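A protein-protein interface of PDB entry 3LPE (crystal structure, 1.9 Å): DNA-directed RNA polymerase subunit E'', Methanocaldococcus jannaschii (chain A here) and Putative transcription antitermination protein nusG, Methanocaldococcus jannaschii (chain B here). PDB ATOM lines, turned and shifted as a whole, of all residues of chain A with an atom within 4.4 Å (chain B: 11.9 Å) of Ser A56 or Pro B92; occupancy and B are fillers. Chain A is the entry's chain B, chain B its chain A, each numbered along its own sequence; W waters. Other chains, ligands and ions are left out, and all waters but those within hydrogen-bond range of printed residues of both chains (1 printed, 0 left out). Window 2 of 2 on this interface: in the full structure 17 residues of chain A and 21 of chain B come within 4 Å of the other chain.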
ATOM      1  N   LYS A   8     -31.056 -12.066  13.941  1.00  0.00           N
ATOM      2  CA  LYS A   8     -30.742 -13.251  14.779  1.00  0.00           C
ATOM      3  C   LYS A   8     -30.527 -12.970  16.266  1.00  0.00           C
ATOM      4  O   LYS A   8     -30.219 -13.883  17.061  1.00  0.00           O
ATOM      5  CB  LYS A   8     -29.562 -14.046  14.184  1.00  0.00           C
ATOM      6  CG  LYS A   8     -29.873 -14.634  12.826  1.00  0.00           C
ATOM      7  CD  LYS A   8     -28.730 -15.479  12.254  1.00  0.00           C
ATOM      8  CE  LYS A   8     -27.640 -14.619  11.654  1.00  0.00           C
ATOM      9  NZ  LYS A   8     -26.866 -15.371  10.623  1.00  0.00           N
ATOM     10  N   TRP A  27     -34.691 -21.454  15.768  1.00  0.00           N
ATOM     11  CA  TRP A  27     -33.347 -20.958  15.552  1.00  0.00           C
ATOM     12  C   TRP A  27     -32.333 -21.996  16.007  1.00  0.00           C
ATOM     13  O   TRP A  27     -32.641 -22.878  16.814  1.00  0.00           O
ATOM     14  CB  TRP A  27     -33.118 -19.628  16.285  1.00  0.00           C
ATOM     15  CG  TRP A  27     -33.297 -19.693  17.783  1.00  0.00           C
ATOM     16  CD1 TRP A  27     -34.445 -19.472  18.473  1.00  0.00           C
ATOM     17  CD2 TRP A  27     -32.289 -19.999  18.767  1.00  0.00           C
ATOM     18  NE1 TRP A  27     -34.229 -19.631  19.816  1.00  0.00           N
ATOM     19  CE2 TRP A  27     -32.911 -19.949  20.026  1.00  0.00           C
ATOM     20  CE3 TRP A  27     -30.929 -20.311  18.698  1.00  0.00           C
ATOM     21  CZ2 TRP A  27     -32.220 -20.191  21.215  1.00  0.00           C
ATOM     22  CZ3 TRP A  27     -30.242 -20.559  19.879  1.00  0.00           C
ATOM     23  CH2 TRP A  27     -30.892 -20.499  21.122  1.00  0.00           C
ATOM     24  N   ILE A  28     -31.125 -21.865  15.484  1.00  0.00           N
ATOM     25  CA  ILE A  28     -30.044 -22.830  15.688  1.00  0.00           C
ATOM     26  C   ILE A  28     -28.705 -22.144  15.874  1.00  0.00           C
ATOM     27  O   ILE A  28     -28.380 -21.207  15.158  1.00  0.00           O
ATOM     28  CB  ILE A  28     -29.947 -23.783  14.475  1.00  0.00           C
ATOM     29  CG1 ILE A  28     -31.114 -24.765  14.511  1.00  0.00           C
ATOM     30  CG2 ILE A  28     -28.633 -24.536  14.476  1.00  0.00           C
ATOM     31  CD1 ILE A  28     -31.294 -25.403  15.874  1.00  0.00           C
ATOM     32  N   ALA A  54     -28.461 -16.147  17.402  1.00  0.00           N
ATOM     33  CA  ALA A  54     -28.544 -17.490  16.818  1.00  0.00           C
ATOM     34  C   ALA A  54     -27.610 -17.518  15.619  1.00  0.00           C
ATOM     35  O   ALA A  54     -27.216 -16.452  15.142  1.00  0.00           O
ATOM     36  CB  ALA A  54     -29.985 -17.793  16.414  1.00  0.00           C
ATOM     37  N   LEU A  55     -27.212 -18.708  15.144  1.00  0.00           N
ATOM     38  CA  LEU A  55     -26.421 -18.781  13.919  1.00  0.00           C
ATOM     39  C   LEU A  55     -27.293 -18.838  12.673  1.00  0.00           C
ATOM     40  O   LEU A  55     -26.902 -18.384  11.600  1.00  0.00           O
ATOM     41  CB  LEU A  55     -25.443 -19.963  13.944  1.00  0.00           C
ATOM     42  CG  LEU A  55     -24.416 -19.861  15.063  1.00  0.00           C
ATOM     43  CD1 LEU A  55     -23.480 -21.067  15.024  1.00  0.00           C
ATOM     44  CD2 LEU A  55     -23.633 -18.556  14.938  1.00  0.00           C
ATOM     45  N   SER A  56     -28.486 -19.387  12.822  1.00  0.00           N
ATOM     46  CA  SER A  56     -29.458 -19.383  11.740  1.00  0.00           C
ATOM     47  C   SER A  56     -30.866 -19.397  12.318  1.00  0.00           C
ATOM     48  O   SER A  56     -31.101 -19.899  13.426  1.00  0.00           O
ATOM     49  CB  SER A  56     -29.254 -20.593  10.790  1.00  0.00           C
ATOM     50  OG  SER A  56     -29.740 -21.781  11.360  1.00  0.00           O
ATOM     51  N   VAL A  57     -31.803 -18.851  11.559  1.00  0.00           N
ATOM     52  CA  VAL A  57     -33.172 -18.727  12.020  1.00  0.00           C
ATOM     53  C   VAL A  57     -34.106 -18.925  10.856  1.00  0.00           C
ATOM     54  O   VAL A  57     -33.786 -18.550   9.725  1.00  0.00           O
ATOM     55  CB  VAL A  57     -33.472 -17.311  12.574  1.00  0.00           C
ATOM     56  CG1 VAL A  57     -34.813 -17.315  13.286  1.00  0.00           C
ATOM     57  CG2 VAL A  57     -32.374 -16.836  13.501  1.00  0.00           C
ATOM     58  N   LYS B  23     -24.457 -24.887  24.789  1.00  0.00           N
ATOM     59  CA  LYS B  23     -25.125 -23.593  24.988  1.00  0.00           C
ATOM     60  C   LYS B  23     -25.203 -23.225  26.462  1.00  0.00           C
ATOM     61  O   LYS B  23     -24.999 -22.067  26.821  1.00  0.00           O
ATOM     62  CB  LYS B  23     -26.532 -23.611  24.384  1.00  0.00           C
ATOM     63  CG  LYS B  23     -26.564 -23.474  22.870  1.00  0.00           C
ATOM     64  CD  LYS B  23     -27.982 -23.730  22.365  1.00  0.00           C
ATOM     65  CE  LYS B  23     -28.085 -23.645  20.871  1.00  0.00           C
ATOM     66  NZ  LYS B  23     -29.496 -23.858  20.447  1.00  0.00           N
ATOM     67  N   LEU B  44     -18.779 -19.070  21.091  1.00  0.00           N
ATOM     68  CA  LEU B  44     -19.544 -19.611  19.974  1.00  0.00           C
ATOM     69  C   LEU B  44     -19.841 -21.096  20.203  1.00  0.00           C
ATOM     70  O   LEU B  44     -18.917 -21.893  20.442  1.00  0.00           O
ATOM     71  CB  LEU B  44     -18.755 -19.413  18.664  1.00  0.00           C
ATOM     72  CG  LEU B  44     -19.223 -20.198  17.448  1.00  0.00           C
ATOM     73  CD1 LEU B  44     -20.405 -19.521  16.846  1.00  0.00           C
ATOM     74  CD2 LEU B  44     -18.111 -20.329  16.434  1.00  0.00           C
ATOM     75  N   ALA B  45     -21.121 -21.450  20.151  1.00  0.00           N
ATOM     76  CA  ALA B  45     -21.550 -22.832  20.301  1.00  0.00           C
ATOM     77  C   ALA B  45     -22.303 -23.233  19.055  1.00  0.00           C
ATOM     78  O   ALA B  45     -23.445 -22.831  18.869  1.00  0.00           O
ATOM     79  CB  ALA B  45     -22.422 -23.011  21.549  1.00  0.00           C
ATOM     80  N   SER B  46     -21.647 -24.004  18.194  1.00  0.00           N
ATOM     81  CA  SER B  46     -22.222 -24.452  16.926  1.00  0.00           C
ATOM     82  C   SER B  46     -22.792 -25.858  17.046  1.00  0.00           C
ATOM     83  O   SER B  46     -22.156 -26.733  17.646  1.00  0.00           O
ATOM     84  CB  SER B  46     -21.136 -24.459  15.850  1.00  0.00           C
ATOM     85  OG  SER B  46     -21.561 -25.180  14.707  1.00  0.00           O
ATOM     86  N   GLU B  47     -23.967 -26.075  16.458  1.00  0.00           N
ATOM     87  CA  GLU B  47     -24.608 -27.382  16.470  1.00  0.00           C
ATOM     88  C   GLU B  47     -23.758 -28.392  15.722  1.00  0.00           C
ATOM     89  O   GLU B  47     -23.885 -29.589  15.929  1.00  0.00           O
ATOM     90  CB  GLU B  47     -26.003 -27.318  15.841  1.00  0.00           C
ATOM     91  CG  GLU B  47     -27.038 -26.660  16.724  1.00  0.00           C
ATOM     92  CD  GLU B  47     -27.162 -27.340  18.072  1.00  0.00           C
ATOM     93  OE1 GLU B  47     -27.300 -26.631  19.094  1.00  0.00           O
ATOM     94  OE2 GLU B  47     -27.114 -28.586  18.112  1.00  0.00           O
ATOM     95  N   SER B  48     -22.888 -27.913  14.846  1.00  0.00           N
ATOM     96  CA  SER B  48     -22.101 -28.824  14.039  1.00  0.00           C
ATOM     97  C   SER B  48     -20.796 -29.140  14.763  1.00  0.00           C
ATOM     98  O   SER B  48     -19.905 -29.809  14.233  1.00  0.00           O
ATOM     99  CB  SER B  48     -21.862 -28.238  12.642  1.00  0.00           C
ATOM    100  OG  SER B  48     -20.778 -27.344  12.672  1.00  0.00           O
ATOM    101  N   LEU B  49     -20.703 -28.677  16.000  1.00  0.00           N
ATOM    102  CA  LEU B  49     -19.510 -28.911  16.804  1.00  0.00           C
ATOM    103  C   LEU B  49     -19.871 -29.349  18.213  1.00  0.00           C
ATOM    104  O   LEU B  49     -19.732 -28.586  19.165  1.00  0.00           O
ATOM    105  CB  LEU B  49     -18.651 -27.653  16.862  1.00  0.00           C
ATOM    106  CG  LEU B  49     -17.304 -27.828  17.550  1.00  0.00           C
ATOM    107  CD1 LEU B  49     -16.573 -29.005  16.923  1.00  0.00           C
ATOM    108  CD2 LEU B  49     -16.479 -26.550  17.442  1.00  0.00           C
ATOM    109  N   GLU B  85     -11.029 -21.248  10.176  1.00  0.00           N
ATOM    110  CA  GLU B  85     -11.632 -22.532  10.552  1.00  0.00           C
ATOM    111  C   GLU B  85     -12.982 -22.340  11.232  1.00  0.00           C
ATOM    112  O   GLU B  85     -13.782 -23.263  11.342  1.00  0.00           O
ATOM    113  CB  GLU B  85     -10.667 -23.375  11.421  1.00  0.00           C
ATOM    114  CG  GLU B  85      -9.436 -23.842  10.627  1.00  0.00           C
ATOM    115  CD  GLU B  85      -8.429 -24.664  11.439  1.00  0.00           C
ATOM    116  OE1 GLU B  85      -8.669 -24.907  12.636  1.00  0.00           O
ATOM    117  OE2 GLU B  85      -7.388 -25.053  10.862  1.00  0.00           O
ATOM    118  N   ILE B  86     -13.248 -21.110  11.648  1.00  0.00           N
ATOM    119  CA  ILE B  86     -14.480 -20.762  12.331  1.00  0.00           C
ATOM    120  C   ILE B  86     -15.575 -20.223  11.403  1.00  0.00           C
ATOM    121  O   ILE B  86     -16.756 -20.484  11.610  1.00  0.00           O
ATOM    122  CB  ILE B  86     -14.167 -19.733  13.434  1.00  0.00           C
ATOM    123  CG1 ILE B  86     -13.424 -20.427  14.576  1.00  0.00           C
ATOM    124  CG2 ILE B  86     -15.426 -19.036  13.931  1.00  0.00           C
ATOM    125  CD1 ILE B  86     -13.043 -19.505  15.692  1.00  0.00           C
ATOM    126  N   GLU B  87     -15.178 -19.471  10.379  1.00  0.00           N
ATOM    127  CA  GLU B  87     -16.118 -18.834   9.468  1.00  0.00           C
ATOM    128  C   GLU B  87     -17.233 -19.733   8.915  1.00  0.00           C
ATOM    129  O   GLU B  87     -18.395 -19.308   8.864  1.00  0.00           O
ATOM    130  CB  GLU B  87     -15.371 -18.121   8.329  1.00  0.00           C
ATOM    131  CG  GLU B  87     -14.453 -17.014   8.830  1.00  0.00           C
ATOM    132  CD  GLU B  87     -13.772 -16.253   7.708  1.00  0.00           C
ATOM    133  OE1 GLU B  87     -14.449 -15.935   6.708  1.00  0.00           O
ATOM    134  OE2 GLU B  87     -12.564 -15.963   7.839  1.00  0.00           O
ATOM    135  N   PRO B  88     -16.893 -20.966   8.492  1.00  0.00           N
ATOM    136  CA  PRO B  88     -17.954 -21.841   7.982  1.00  0.00           C
ATOM    137  C   PRO B  88     -19.019 -22.137   9.039  1.00  0.00           C
ATOM    138  O   PRO B  88     -20.162 -22.435   8.689  1.00  0.00           O
ATOM    139  CB  PRO B  88     -17.197 -23.130   7.610  1.00  0.00           C
ATOM    140  CG  PRO B  88     -15.787 -22.701   7.399  1.00  0.00           C
ATOM    141  CD  PRO B  88     -15.570 -21.617   8.418  1.00  0.00           C
ATOM    142  N   LEU B  89     -18.646 -22.064  10.312  1.00  0.00           N
ATOM    143  CA  LEU B  89     -19.609 -22.273  11.390  1.00  0.00           C
ATOM    144  C   LEU B  89     -20.631 -21.136  11.508  1.00  0.00           C
ATOM    145  O   LEU B  89     -21.723 -21.330  12.046  1.00  0.00           O
ATOM    146  CB  LEU B  89     -18.888 -22.466  12.726  1.00  0.00           C
ATOM    147  CG  LEU B  89     -17.930 -23.661  12.746  1.00  0.00           C
ATOM    148  CD1 LEU B  89     -17.243 -23.788  14.090  1.00  0.00           C
ATOM    149  CD2 LEU B  89     -18.689 -24.911  12.415  1.00  0.00           C
ATOM    150  N   LEU B  90     -20.275 -19.965  10.981  1.00  0.00           N
ATOM    151  CA  LEU B  90     -21.107 -18.768  11.102  1.00  0.00           C
ATOM    152  C   LEU B  90     -22.378 -18.831  10.271  1.00  0.00           C
ATOM    153  O   LEU B  90     -23.419 -18.316  10.668  1.00  0.00           O
ATOM    154  CB  LEU B  90     -20.308 -17.523  10.733  1.00  0.00           C
ATOM    155  CG  LEU B  90     -19.743 -16.749  11.920  1.00  0.00           C
ATOM    156  CD1 LEU B  90     -19.489 -17.657  13.096  1.00  0.00           C
ATOM    157  CD2 LEU B  90     -18.472 -16.016  11.519  1.00  0.00           C
ATOM    158  N   THR B  91     -22.291 -19.455   9.108  1.00  0.00           N
ATOM    159  CA  THR B  91     -23.485 -19.702   8.324  1.00  0.00           C
ATOM    160  C   THR B  91     -23.704 -21.204   8.240  1.00  0.00           C
ATOM    161  O   THR B  91     -23.225 -21.850   7.312  1.00  0.00           O
ATOM    162  CB  THR B  91     -23.384 -19.099   6.918  1.00  0.00           C
ATOM    163  OG1 THR B  91     -22.812 -17.791   7.009  1.00  0.00           O
ATOM    164  CG2 THR B  91     -24.772 -18.999   6.283  1.00  0.00           C
ATOM    165  N   PRO B  92     -24.429 -21.759   9.224  1.00  0.00           N
ATOM    166  CA  PRO B  92     -24.681 -23.200   9.357  1.00  0.00           C
ATOM    167  C   PRO B  92     -25.050 -23.882   8.030  1.00  0.00           C
ATOM    168  O   PRO B  92     -24.259 -24.641   7.463  1.00  0.00           O
ATOM    169  CB  PRO B  92     -25.860 -23.258  10.331  1.00  0.00           C
ATOM    170  CG  PRO B  92     -25.730 -22.022  11.164  1.00  0.00           C
ATOM    171  CD  PRO B  92     -25.063 -20.975  10.304  1.00  0.00           C
ATOM    172  OXT PRO B  92     -26.142 -23.704   7.482  1.00  0.00           O
HETATM  173  O   HOH W   1     -24.472 -16.388  11.787  1.00  0.00           O
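NZ of Lys B23 touches CZ3 of Trp A27 (3.4 Å). CG of Glu B47 touches CG2 of Ile A28 (3.5 Å). Leu A55 touches Leu B44. CD1 of Leu A55 touches O of Leu B89, at 3.5 Å. O of Leu B90 touches O of Leu A55, 3.6 Å away. O of Leu A55 touches CD of Pro B92, 3.4 Å away. Pro B92 touches Ser A56.
Of the 7 printed residues of chain A, 4 touch a printed residue of chain B. Printed residues of chain B that touch a printed residue of chain A: Lys B23, Leu B44, Glu B47, Leu B89, Leu B90 and Pro B92. Hydrophobic or aromatic side chains of chain B that line the printed part of chain A: Leu B44 and Pro B92. Among the printed residues, 7 pairs touch across the chains. Among the printed residues, no Asp or Glu carboxylate lies within 4 Å of a Lys or Arg side-chain nitrogen of the other chain.
Water W1 lies within hydrogen-bond range of O of Leu B90 (2.5 Å), NZ of Lys A8 (2.8 Å) and O of Leu A55 (3.2 Å).
Ile A28 touches one residue of chain B. No residue of chain B comes within 4 Å of Ala A54. Of chain B, only Pro B92 (3.8 Å) comes within 4 Å of Ser A56. Printed residues of chain A within 4 Å of Leu B44: Leu A55 (3.9 Å). Of the printed residues of chain A, Glu B47 touches Ile A28 (3.5 Å). Pro B88 touches none of the printed residues of chain A. Of the printed residues of chain A, Leu B89 touches Leu A55. Of the printed residues of chain A, Pro B92 touches Leu A55 (3.4 Å) and Ser A56 (3.8 Å). The nearest residue of chain B that does not touch Ser A56 is Leu B90 (5.6 Å). The nearest printed residue of chain A that does not touch Pro B92 is Ile A28 (4.9 Å).
NZ of Lys B23 is in salt-bridge range of OE1 of Glu B47 (3.8 Å). NZ of Lys A8 lies within hydrogen-bond range of O of Leu A55 (3.2 Å). The backbone carbonyl oxygen (O) of Ile A28 lies within hydrogen-bond range of the backbone NH (N) of Leu A55, 2.8 Å away. N of Ile A28 sits at hydrogen-bond distance from O of Ser A56 (2.8 Å).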
